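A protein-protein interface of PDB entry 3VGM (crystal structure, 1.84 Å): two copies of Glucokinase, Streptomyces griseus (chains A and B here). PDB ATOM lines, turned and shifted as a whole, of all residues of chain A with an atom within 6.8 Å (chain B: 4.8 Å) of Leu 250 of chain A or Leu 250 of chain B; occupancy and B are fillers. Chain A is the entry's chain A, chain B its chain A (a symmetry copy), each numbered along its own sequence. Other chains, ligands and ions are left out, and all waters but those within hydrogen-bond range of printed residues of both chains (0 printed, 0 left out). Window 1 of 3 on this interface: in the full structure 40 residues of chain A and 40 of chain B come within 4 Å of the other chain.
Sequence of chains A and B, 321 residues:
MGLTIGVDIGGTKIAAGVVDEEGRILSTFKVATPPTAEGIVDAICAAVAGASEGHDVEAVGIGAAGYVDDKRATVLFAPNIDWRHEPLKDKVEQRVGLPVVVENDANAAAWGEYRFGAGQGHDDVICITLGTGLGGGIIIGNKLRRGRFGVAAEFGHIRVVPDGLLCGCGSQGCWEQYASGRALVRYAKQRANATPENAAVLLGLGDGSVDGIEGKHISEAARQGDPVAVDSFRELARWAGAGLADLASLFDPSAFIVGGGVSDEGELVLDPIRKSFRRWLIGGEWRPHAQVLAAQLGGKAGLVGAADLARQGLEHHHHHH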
ATOM      1  N   ILE A 138       4.700 -13.675 -27.273  1.00  0.00           N
ATOM      2  CA  ILE A 138       4.812 -12.240 -27.369  1.00  0.00           C
ATOM      3  C   ILE A 138       6.190 -11.784 -26.940  1.00  0.00           C
ATOM      4  O   ILE A 138       6.604 -12.046 -25.802  1.00  0.00           O
ATOM      5  CB  ILE A 138       3.775 -11.576 -26.405  1.00  0.00           C
ATOM      6  CG1 ILE A 138       2.340 -11.939 -26.828  1.00  0.00           C
ATOM      7  CG2 ILE A 138       3.974 -10.044 -26.315  1.00  0.00           C
ATOM      8  CD1 ILE A 138       1.321 -11.815 -25.656  1.00  0.00           C
ATOM      9  N   ARG A 145       6.840 -11.983 -22.902  1.00  0.00           N
ATOM     10  CA  ARG A 145       5.817 -11.491 -21.974  1.00  0.00           C
ATOM     11  C   ARG A 145       4.814 -12.627 -21.699  1.00  0.00           C
ATOM     12  O   ARG A 145       4.043 -13.013 -22.579  1.00  0.00           O
ATOM     13  CB  ARG A 145       5.084 -10.259 -22.573  1.00  0.00           C
ATOM     14  CG  ARG A 145       6.026  -9.142 -23.018  1.00  0.00           C
ATOM     15  CD  ARG A 145       6.861  -8.616 -21.831  1.00  0.00           C
ATOM     16  NE  ARG A 145       7.761  -7.534 -22.241  1.00  0.00           N
ATOM     17  CZ  ARG A 145       8.287  -6.625 -21.419  1.00  0.00           C
ATOM     18  NH1 ARG A 145       8.005  -6.627 -20.110  1.00  0.00           N
ATOM     19  NH2 ARG A 145       9.136  -5.721 -21.912  1.00  0.00           N
ATOM     20  N   GLY A 147       2.609 -12.489 -19.117  1.00  0.00           N
ATOM     21  CA  GLY A 147       1.446 -11.945 -18.395  1.00  0.00           C
ATOM     22  C   GLY A 147       1.600 -12.062 -16.880  1.00  0.00           C
ATOM     23  O   GLY A 147       2.565 -12.664 -16.374  1.00  0.00           O
ATOM     24  N   VAL A 151      -0.060 -16.884 -18.228  1.00  0.00           N
ATOM     25  CA  VAL A 151      -0.942 -17.472 -19.266  1.00  0.00           C
ATOM     26  C   VAL A 151      -1.249 -16.558 -20.461  1.00  0.00           C
ATOM     27  O   VAL A 151      -2.278 -16.751 -21.162  1.00  0.00           O
ATOM     28  CB  VAL A 151      -2.286 -18.005 -18.635  1.00  0.00           C
ATOM     29  CG1 VAL A 151      -3.050 -18.864 -19.629  1.00  0.00           C
ATOM     30  CG2 VAL A 151      -1.989 -18.823 -17.374  1.00  0.00           C
ATOM     31  N   ALA A 152      -0.366 -15.597 -20.734  1.00  0.00           N
ATOM     32  CA  ALA A 152      -0.541 -14.735 -21.912  1.00  0.00           C
ATOM     33  C   ALA A 152      -0.310 -15.530 -23.191  1.00  0.00           C
ATOM     34  O   ALA A 152       0.227 -16.659 -23.142  1.00  0.00           O
ATOM     35  CB  ALA A 152       0.440 -13.558 -21.853  1.00  0.00           C
ATOM     36  N   ALA A 153      -0.687 -14.929 -24.321  1.00  0.00           N
ATOM     37  CA  ALA A 153      -0.447 -15.497 -25.650  1.00  0.00           C
ATOM     38  C   ALA A 153      -1.079 -16.886 -25.788  1.00  0.00           C
ATOM     39  O   ALA A 153      -0.519 -17.774 -26.475  1.00  0.00           O
ATOM     40  CB  ALA A 153       1.087 -15.534 -25.994  1.00  0.00           C
ATOM     41  N   GLU A 154      -2.256 -17.081 -25.181  1.00  0.00           N
ATOM     42  CA  GLU A 154      -3.097 -18.217 -25.591  1.00  0.00           C
ATOM     43  C   GLU A 154      -3.894 -17.841 -26.855  1.00  0.00           C
ATOM     44  O   GLU A 154      -5.141 -17.810 -26.857  1.00  0.00           O
ATOM     45  CB  GLU A 154      -4.019 -18.688 -24.454  1.00  0.00           C
ATOM     46  CG  GLU A 154      -3.222 -19.580 -23.431  1.00  0.00           C
ATOM     47  CD  GLU A 154      -2.701 -20.876 -24.075  1.00  0.00           C
ATOM     48  OE1 GLU A 154      -3.407 -21.455 -24.939  1.00  0.00           O
ATOM     49  OE2 GLU A 154      -1.594 -21.340 -23.715  1.00  0.00           O
ATOM     50  N   PHE A 155      -3.157 -17.541 -27.923  1.00  0.00           N
ATOM     51  CA  PHE A 155      -3.770 -17.120 -29.199  1.00  0.00           C
ATOM     52  C   PHE A 155      -4.765 -18.125 -29.763  1.00  0.00           C
ATOM     53  O   PHE A 155      -5.710 -17.735 -30.443  1.00  0.00           O
ATOM     54  CB  PHE A 155      -2.675 -16.909 -30.250  1.00  0.00           C
ATOM     55  CG  PHE A 155      -1.705 -15.803 -29.901  1.00  0.00           C
ATOM     56  CD1 PHE A 155      -2.131 -14.644 -29.299  1.00  0.00           C
ATOM     57  CD2 PHE A 155      -0.373 -15.913 -30.208  1.00  0.00           C
ATOM     58  CE1 PHE A 155      -1.224 -13.599 -28.987  1.00  0.00           C
ATOM     59  CE2 PHE A 155       0.546 -14.860 -29.905  1.00  0.00           C
ATOM     60  CZ  PHE A 155       0.109 -13.713 -29.295  1.00  0.00           C
ATOM     61  N   ILE A 158      -8.539 -17.358 -28.520  1.00  0.00           N
ATOM     62  CA  ILE A 158      -9.360 -16.152 -28.735  1.00  0.00           C
ATOM     63  C   ILE A 158     -10.566 -16.539 -29.611  1.00  0.00           C
ATOM     64  O   ILE A 158     -10.442 -17.374 -30.523  1.00  0.00           O
ATOM     65  CB  ILE A 158      -8.558 -15.002 -29.392  1.00  0.00           C
ATOM     66  CG1 ILE A 158      -8.051 -15.402 -30.771  1.00  0.00           C
ATOM     67  CG2 ILE A 158      -7.382 -14.592 -28.493  1.00  0.00           C
ATOM     68  CD1 ILE A 158      -7.395 -14.250 -31.583  1.00  0.00           C
ATOM     69  N   GLY A 243      -6.804 -13.462 -38.412  1.00  0.00           N
ATOM     70  CA  GLY A 243      -6.321 -13.454 -37.027  1.00  0.00           C
ATOM     71  C   GLY A 243      -5.043 -12.641 -36.865  1.00  0.00           C
ATOM     72  O   GLY A 243      -4.901 -11.910 -35.873  1.00  0.00           O
ATOM     73  N   LEU A 244      -4.113 -12.739 -37.822  1.00  0.00           N
ATOM     74  CA  LEU A 244      -2.910 -11.883 -37.760  1.00  0.00           C
ATOM     75  C   LEU A 244      -3.281 -10.407 -37.834  1.00  0.00           C
ATOM     76  O   LEU A 244      -2.710  -9.568 -37.126  1.00  0.00           O
ATOM     77  CB  LEU A 244      -1.895 -12.208 -38.853  1.00  0.00           C
ATOM     78  CG  LEU A 244      -1.158 -13.536 -38.789  1.00  0.00           C
ATOM     79  CD1 LEU A 244      -0.195 -13.621 -40.000  1.00  0.00           C
ATOM     80  CD2 LEU A 244      -0.400 -13.698 -37.454  1.00  0.00           C
ATOM     81  N   ALA A 245      -4.238 -10.090 -38.687  1.00  0.00           N
ATOM     82  CA  ALA A 245      -4.732  -8.707 -38.766  1.00  0.00           C
ATOM     83  C   ALA A 245      -5.265  -8.201 -37.409  1.00  0.00           C
ATOM     84  O   ALA A 245      -4.969  -7.073 -37.011  1.00  0.00           O
ATOM     85  CB  ALA A 245      -5.812  -8.568 -39.877  1.00  0.00           C
ATOM     86  N   ASP A 246      -6.027  -9.028 -36.692  1.00  0.00           N
ATOM     87  CA  ASP A 246      -6.491  -8.671 -35.329  1.00  0.00           C
ATOM     88  C   ASP A 246      -5.304  -8.474 -34.379  1.00  0.00           C
ATOM     89  O   ASP A 246      -5.284  -7.538 -33.577  1.00  0.00           O
ATOM     90  CB  ASP A 246      -7.378  -9.781 -34.729  1.00  0.00           C
ATOM     91  CG  ASP A 246      -8.768  -9.848 -35.357  1.00  0.00           C
ATOM     92  OD1 ASP A 246      -9.216  -8.857 -36.024  1.00  0.00           O
ATOM     93  OD2 ASP A 246      -9.424 -10.905 -35.169  1.00  0.00           O
ATOM     94  N   LEU A 247      -4.325  -9.377 -34.451  1.00  0.00           N
ATOM     95  CA  LEU A 247      -3.135  -9.225 -33.609  1.00  0.00           C
ATOM     96  C   LEU A 247      -2.383  -7.950 -33.926  1.00  0.00           C
ATOM     97  O   LEU A 247      -1.772  -7.396 -33.031  1.00  0.00           O
ATOM     98  CB  LEU A 247      -2.192 -10.425 -33.738  1.00  0.00           C
ATOM     99  CG  LEU A 247      -2.814 -11.762 -33.314  1.00  0.00           C
ATOM    100  CD1 LEU A 247      -1.798 -12.912 -33.507  1.00  0.00           C
ATOM    101  CD2 LEU A 247      -3.244 -11.704 -31.866  1.00  0.00           C
ATOM    102  N   ALA A 248      -2.389  -7.515 -35.192  1.00  0.00           N
ATOM    103  CA  ALA A 248      -1.742  -6.233 -35.534  1.00  0.00           C
ATOM    104  C   ALA A 248      -2.469  -5.066 -34.853  1.00  0.00           C
ATOM    105  O   ALA A 248      -1.824  -4.133 -34.404  1.00  0.00           O
ATOM    106  CB  ALA A 248      -1.713  -5.997 -37.080  1.00  0.00           C
ATOM    107  N   SER A 249      -3.799  -5.120 -34.805  1.00  0.00           N
ATOM    108  CA  SER A 249      -4.559  -4.064 -34.100  1.00  0.00           C
ATOM    109  C   SER A 249      -4.321  -4.078 -32.607  1.00  0.00           C
ATOM    110  O   SER A 249      -4.401  -3.023 -31.965  1.00  0.00           O
ATOM    111  CB  SER A 249      -6.047  -4.197 -34.373  1.00  0.00           C
ATOM    112  OG  SER A 249      -6.247  -3.695 -35.682  1.00  0.00           O
ATOM    113  N   LEU A 250      -4.017  -5.255 -32.063  1.00  0.00           N
ATOM    114  CA  LEU A 250      -3.749  -5.377 -30.622  1.00  0.00           C
ATOM    115  C   LEU A 250      -2.333  -4.969 -30.260  1.00  0.00           C
ATOM    116  O   LEU A 250      -2.128  -4.103 -29.398  1.00  0.00           O
ATOM    117  CB  LEU A 250      -4.045  -6.805 -30.135  1.00  0.00           C
ATOM    118  CG  LEU A 250      -5.532  -7.238 -30.235  1.00  0.00           C
ATOM    119  CD1 LEU A 250      -5.668  -8.745 -30.473  1.00  0.00           C
ATOM    120  CD2 LEU A 250      -6.263  -6.876 -28.995  1.00  0.00           C
ATOM    121  N   PHE A 251      -1.349  -5.590 -30.914  1.00  0.00           N
ATOM    122  CA  PHE A 251       0.050  -5.429 -30.512  1.00  0.00           C
ATOM    123  C   PHE A 251       0.883  -4.504 -31.397  1.00  0.00           C
ATOM    124  O   PHE A 251       1.920  -4.010 -30.951  1.00  0.00           O
ATOM    125  CB  PHE A 251       0.740  -6.785 -30.549  1.00  0.00           C
ATOM    126  CG  PHE A 251       0.231  -7.738 -29.541  1.00  0.00           C
ATOM    127  CD1 PHE A 251       0.683  -7.669 -28.227  1.00  0.00           C
ATOM    128  CD2 PHE A 251      -0.683  -8.711 -29.895  1.00  0.00           C
ATOM    129  CE1 PHE A 251       0.248  -8.578 -27.282  1.00  0.00           C
ATOM    130  CE2 PHE A 251      -1.149  -9.619 -28.937  1.00  0.00           C
ATOM    131  CZ  PHE A 251      -0.684  -9.546 -27.631  1.00  0.00           C
ATOM    132  N   ASP A 252       0.441  -4.303 -32.637  1.00  0.00           N
ATOM    133  CA  ASP A 252       1.171  -3.490 -33.635  1.00  0.00           C
ATOM    134  C   ASP A 252       2.685  -3.802 -33.673  1.00  0.00           C
ATOM    135  O   ASP A 252       3.499  -2.897 -33.519  1.00  0.00           O
ATOM    136  CB  ASP A 252       0.949  -1.993 -33.365  1.00  0.00           C
ATOM    137  CG  ASP A 252       1.474  -1.099 -34.503  1.00  0.00           C
ATOM    138  OD1 ASP A 252       1.305  -1.473 -35.690  1.00  0.00           O
ATOM    139  OD2 ASP A 252       2.016  -0.010 -34.203  1.00  0.00           O
ATOM    140  N   PRO A 253       3.062  -5.082 -33.868  1.00  0.00           N
ATOM    141  CA  PRO A 253       4.493  -5.428 -33.810  1.00  0.00           C
ATOM    142  C   PRO A 253       5.243  -5.003 -35.080  1.00  0.00           C
ATOM    143  O   PRO A 253       4.622  -4.645 -36.077  1.00  0.00           O
ATOM    144  CB  PRO A 253       4.465  -6.962 -33.723  1.00  0.00           C
ATOM    145  CG  PRO A 253       3.255  -7.329 -34.551  1.00  0.00           C
ATOM    146  CD  PRO A 253       2.228  -6.219 -34.308  1.00  0.00           C
ATOM    147  N   ARG A 287      -1.399   3.208 -42.003  1.00  0.00           N
ATOM    148  CA  ARG A 287      -0.433   2.761 -41.013  1.00  0.00           C
ATOM    149  C   ARG A 287       0.605   1.856 -41.692  1.00  0.00           C
ATOM    150  O   ARG A 287       0.294   1.216 -42.710  1.00  0.00           O
ATOM    151  CB  ARG A 287      -1.161   1.971 -39.895  1.00  0.00           C
ATOM    152  CG  ARG A 287      -1.534   0.532 -40.355  1.00  0.00           C
ATOM    153  CD  ARG A 287      -2.523  -0.160 -39.490  1.00  0.00           C
ATOM    154  NE  ARG A 287      -1.878  -0.686 -38.297  1.00  0.00           N
ATOM    155  CZ  ARG A 287      -2.501  -1.385 -37.370  1.00  0.00           C
ATOM    156  NH1 ARG A 287      -1.808  -1.806 -36.309  1.00  0.00           N
ATOM    157  NH2 ARG A 287      -3.814  -1.651 -37.489  1.00  0.00           N
ATOM    158  N   ILE B 138      -2.628  -0.379 -23.263  1.00  0.00           N
ATOM    159  CA  ILE B 138      -1.883  -1.482 -22.703  1.00  0.00           C
ATOM    160  C   ILE B 138      -0.785  -0.976 -21.795  1.00  0.00           C
ATOM    161  O   ILE B 138       0.086  -0.215 -22.240  1.00  0.00           O
ATOM    162  CB  ILE B 138      -1.205  -2.285 -23.862  1.00  0.00           C
ATOM    163  CG1 ILE B 138      -2.272  -2.893 -24.790  1.00  0.00           C
ATOM    164  CG2 ILE B 138      -0.236  -3.363 -23.321  1.00  0.00           C
ATOM    165  CD1 ILE B 138      -1.722  -3.200 -26.215  1.00  0.00           C
ATOM    166  N   ALA B 152      -0.727   0.314 -31.510  1.00  0.00           N
ATOM    167  CA  ALA B 152      -1.211  -0.803 -30.688  1.00  0.00           C
ATOM    168  C   ALA B 152      -2.508  -0.423 -29.984  1.00  0.00           C
ATOM    169  O   ALA B 152      -2.871   0.774 -29.940  1.00  0.00           O
ATOM    170  CB  ALA B 152      -0.154  -1.190 -29.646  1.00  0.00           C
ATOM    171  N   ALA B 153      -3.177  -1.430 -29.419  1.00  0.00           N
ATOM    172  CA  ALA B 153      -4.384  -1.238 -28.613  1.00  0.00           C
ATOM    173  C   ALA B 153      -5.480  -0.519 -29.408  1.00  0.00           C
ATOM    174  O   ALA B 153      -6.255   0.285 -28.837  1.00  0.00           O
ATOM    175  CB  ALA B 153      -4.068  -0.482 -27.270  1.00  0.00           C
ATOM    176  N   PHE B 155      -8.234  -1.741 -29.882  1.00  0.00           N
ATOM    177  CA  PHE B 155      -9.200  -2.775 -29.458  1.00  0.00           C
ATOM    178  C   PHE B 155     -10.548  -2.679 -30.159  1.00  0.00           C
ATOM    179  O   PHE B 155     -11.213  -3.694 -30.349  1.00  0.00           O
ATOM    180  CB  PHE B 155      -9.451  -2.658 -27.951  1.00  0.00           C
ATOM    181  CG  PHE B 155      -8.219  -2.909 -27.111  1.00  0.00           C
ATOM    182  CD1 PHE B 155      -7.308  -3.881 -27.452  1.00  0.00           C
ATOM    183  CD2 PHE B 155      -7.993  -2.193 -25.963  1.00  0.00           C
ATOM    184  CE1 PHE B 155      -6.161  -4.128 -26.654  1.00  0.00           C
ATOM    185  CE2 PHE B 155      -6.843  -2.444 -25.149  1.00  0.00           C
ATOM    186  CZ  PHE B 155      -5.938  -3.409 -25.507  1.00  0.00           C
ATOM    187  N   ILE B 158     -10.664  -4.958 -33.503  1.00  0.00           N
ATOM    188  CA  ILE B 158     -10.493  -6.416 -33.638  1.00  0.00           C
ATOM    189  C   ILE B 158     -11.824  -7.014 -34.132  1.00  0.00           C
ATOM    190  O   ILE B 158     -12.908  -6.551 -33.739  1.00  0.00           O
ATOM    191  CB  ILE B 158     -10.056  -7.085 -32.312  1.00  0.00           C
ATOM    192  CG1 ILE B 158     -11.107  -6.897 -31.228  1.00  0.00           C
ATOM    193  CG2 ILE B 158      -8.707  -6.514 -31.849  1.00  0.00           C
ATOM    194  CD1 ILE B 158     -10.842  -7.690 -29.918  1.00  0.00           C
ATOM    195  N   ASP B 246     -11.326 -12.568 -24.332  1.00  0.00           N
ATOM    196  CA  ASP B 246     -10.292 -12.705 -25.387  1.00  0.00           C
ATOM    197  C   ASP B 246      -9.016 -11.945 -25.008  1.00  0.00           C
ATOM    198  O   ASP B 246      -7.904 -12.442 -25.198  1.00  0.00           O
ATOM    199  CB  ASP B 246     -10.784 -12.131 -26.731  1.00  0.00           C
ATOM    200  CG  ASP B 246     -11.828 -13.008 -27.418  1.00  0.00           C
ATOM    201  OD1 ASP B 246     -11.967 -14.227 -27.067  1.00  0.00           O
ATOM    202  OD2 ASP B 246     -12.510 -12.470 -28.329  1.00  0.00           O
ATOM    203  N   LEU B 247      -9.178 -10.725 -24.494  1.00  0.00           N
ATOM    204  CA  LEU B 247      -8.005  -9.959 -24.060  1.00  0.00           C
ATOM    205  C   LEU B 247      -7.266 -10.655 -22.938  1.00  0.00           C
ATOM    206  O   LEU B 247      -6.061 -10.505 -22.852  1.00  0.00           O
ATOM    207  CB  LEU B 247      -8.383  -8.541 -23.626  1.00  0.00           C
ATOM    208  CG  LEU B 247      -9.027  -7.695 -24.733  1.00  0.00           C
ATOM    209  CD1 LEU B 247      -9.397  -6.294 -24.192  1.00  0.00           C
ATOM    210  CD2 LEU B 247      -8.078  -7.551 -25.901  1.00  0.00           C
ATOM    211  N   ALA B 248      -7.981 -11.371 -22.062  1.00  0.00           N
ATOM    212  CA  ALA B 248      -7.297 -12.136 -21.000  1.00  0.00           C
ATOM    213  C   ALA B 248      -6.441 -13.252 -21.612  1.00  0.00           C
ATOM    214  O   ALA B 248      -5.352 -13.511 -21.124  1.00  0.00           O
ATOM    215  CB  ALA B 248      -8.317 -12.756 -19.990  1.00  0.00           C
ATOM    216  N   SER B 249      -6.947 -13.912 -22.652  1.00  0.00           N
ATOM    217  CA  SER B 249      -6.145 -14.951 -23.334  1.00  0.00           C
ATOM    218  C   SER B 249      -4.943 -14.378 -24.048  1.00  0.00           C
ATOM    219  O   SER B 249      -3.925 -15.069 -24.185  1.00  0.00           O
ATOM    220  CB  SER B 249      -6.996 -15.726 -24.324  1.00  0.00           C
ATOM    221  OG  SER B 249      -7.782 -16.612 -23.547  1.00  0.00           O
ATOM    222  N   LEU B 250      -5.051 -13.125 -24.488  1.00  0.00           N
ATOM    223  CA  LEU B 250      -3.935 -12.464 -25.181  1.00  0.00           C
ATOM    224  C   LEU B 250      -2.897 -11.920 -24.218  1.00  0.00           C
ATOM    225  O   LEU B 250      -1.706 -12.244 -24.326  1.00  0.00           O
ATOM    226  CB  LEU B 250      -4.453 -11.354 -26.108  1.00  0.00           C
ATOM    227  CG  LEU B 250      -5.336 -11.841 -27.287  1.00  0.00           C
ATOM    228  CD1 LEU B 250      -6.378 -10.792 -27.685  1.00  0.00           C
ATOM    229  CD2 LEU B 250      -4.495 -12.160 -28.468  1.00  0.00           C
ATOM    230  N   PHE B 251      -3.340 -11.089 -23.272  1.00  0.00           N
ATOM    231  CA  PHE B 251      -2.411 -10.347 -22.417  1.00  0.00           C
ATOM    232  C   PHE B 251      -2.253 -10.888 -20.998  1.00  0.00           C
ATOM    233  O   PHE B 251      -1.253 -10.590 -20.343  1.00  0.00           O
ATOM    234  CB  PHE B 251      -2.902  -8.913 -22.272  1.00  0.00           C
ATOM    235  CG  PHE B 251      -2.857  -8.140 -23.531  1.00  0.00           C
ATOM    236  CD1 PHE B 251      -1.662  -7.570 -23.955  1.00  0.00           C
ATOM    237  CD2 PHE B 251      -4.000  -7.966 -24.288  1.00  0.00           C
ATOM    238  CE1 PHE B 251      -1.612  -6.810 -25.108  1.00  0.00           C
ATOM    239  CE2 PHE B 251      -3.952  -7.221 -25.471  1.00  0.00           C
ATOM    240  CZ  PHE B 251      -2.755  -6.649 -25.880  1.00  0.00           C
ATOM    241  N   ASP B 252      -3.244 -11.644 -20.531  1.00  0.00           N
ATOM    242  CA  ASP B 252      -3.272 -12.185 -19.154  1.00  0.00           C
ATOM    243  C   ASP B 252      -2.882 -11.134 -18.087  1.00  0.00           C
ATOM    244  O   ASP B 252      -1.966 -11.367 -17.308  1.00  0.00           O
ATOM    245  CB  ASP B 252      -2.349 -13.409 -19.045  1.00  0.00           C
ATOM    246  CG  ASP B 252      -2.517 -14.165 -17.714  1.00  0.00           C
ATOM    247  OD1 ASP B 252      -3.673 -14.305 -17.242  1.00  0.00           O
ATOM    248  OD2 ASP B 252      -1.496 -14.647 -17.171  1.00  0.00           O
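O of Ser 249 of chain B lies within hydrogen-bond range of N of Glu 154 of chain A. O of Ser 249 of chain A lies within hydrogen-bond range of N of Ala 153 of chain B, at 3.2 Å. N of Ala 153 of chain A lies within hydrogen-bond range of O of Ser 249 of chain B, 3.2 Å away. O of Leu 250 of chain B is in hydrogen-bond range of N of Ala 153 of chain A (2.9 Å). N of Ala 153 of chain B lies within hydrogen-bond range of O of Leu 250 of chain A. OD2 of Asp 252 of chain B lies within hydrogen-bond range of N of Val 151 of chain A, 2.9 Å away.
The backbone NH of Arg 145 of chain A lies within hydrogen-bond range of the backbone carbonyl oxygen of Ile 138 of chain A, at 2.9 Å. The side-chain carboxylate (OD1) of Asp 252 of chain A is in salt-bridge range of the guanidinium group (NH1) of Arg 287 of chain A (3.2 Å).
Leu 250 of chain B touches Ile 138 of chain A. O of Phe 251 of chain B touches CA of Gly 147 of chain A (3.6 Å). O of Phe 251 of chain B touches CB of Ala 152 of chain A, 3.7 Å away. Phe 155 of chain A touches Leu 250 of chain B. Ile 158 of chain A touches Asp 246 of chain B (CA to OD1, 3.6 Å). OD1 of Asp 246 of chain A touches CA of Ile 158 of chain B (3.6 Å). Leu 247 of chain A touches Leu 250 of chain B. CG of Leu 250 of chain A touches CG2 of Ile 158 of chain B (3.6 Å). Leu 247 of chain B touches Leu 250 of chain A. CE1 of Phe 251 of chain A touches CE1 of Phe 251 of chain B, at 3.4 Å.
Printed residues of chain B within 4 Å of Val 151 of chain A: Ser 249 and Asp 252. Of the printed residues of chain B, Asp 246 of chain A touches Ile 158 (3.6 Å). Of the printed residues of chain B, Leu 250 of chain A touches Ile 138 (3.3 Å), Ala 152 (3.5 Å), Ala 153 (2.9 Å), Phe 155 (3.5 Å), Ile 158 (3.6 Å), Leu 247 (3.7 Å) and Leu 250 (3.5 Å). Arg 287 of chain A touches none of the printed residues of chain B. Printed residues of chain A within 4 Å of Ile 138 of chain B: Leu 250 (3.3 Å). Of the printed residues of chain A, Leu 247 of chain B touches Leu 250 (3.7 Å). Leu 250 of chain B touches just these residues of chain A: Ile 138, Ala 152, Ala 153, Phe 155, Ile 158, Leu 247 and Leu 250. The nearest residue of chain A that does not touch Leu 250 of chain B is Phe 251 of chain A (4.2 Å).
Of the 21 printed residues of chain A, 14 touch a printed residue of chain B. Along chain A the printed residues that touch a printed residue of chain B span positions 138 to 252. Hydrophobic or aromatic side chains of chain B within 4 Å of the printed part of chain A: Ile 138, Ala 152, Phe 155, Ile 158, Leu 247, Leu 250 and Phe 251. Among the printed residues, no Asp or Glu carboxylate lies within 4 Å of a Lys or Arg side-chain nitrogen of the other chain.
Ala 152 of chain A touches Ser 249 of chain B, and with the chains exchanged Ser 249 of chain A touches Ala 152 of chain B. Phe 155 of chain A touches Leu 250 of chain B, and with the chains exchanged Leu 250 of chain A touches Phe 155 of chain B. Leu 247 of chain A touches Leu 250 of chain B, and with the chains exchanged Leu 250 of chain A touches Leu 247 of chain B. Leu 250 of chain A touches its own counterpart, Leu 250 of chain B. 12 positions are printed for both chains. Of the 29 pairs that touch across the chains among the printed residues, 24 have their exchanged pair printed and touching as well.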
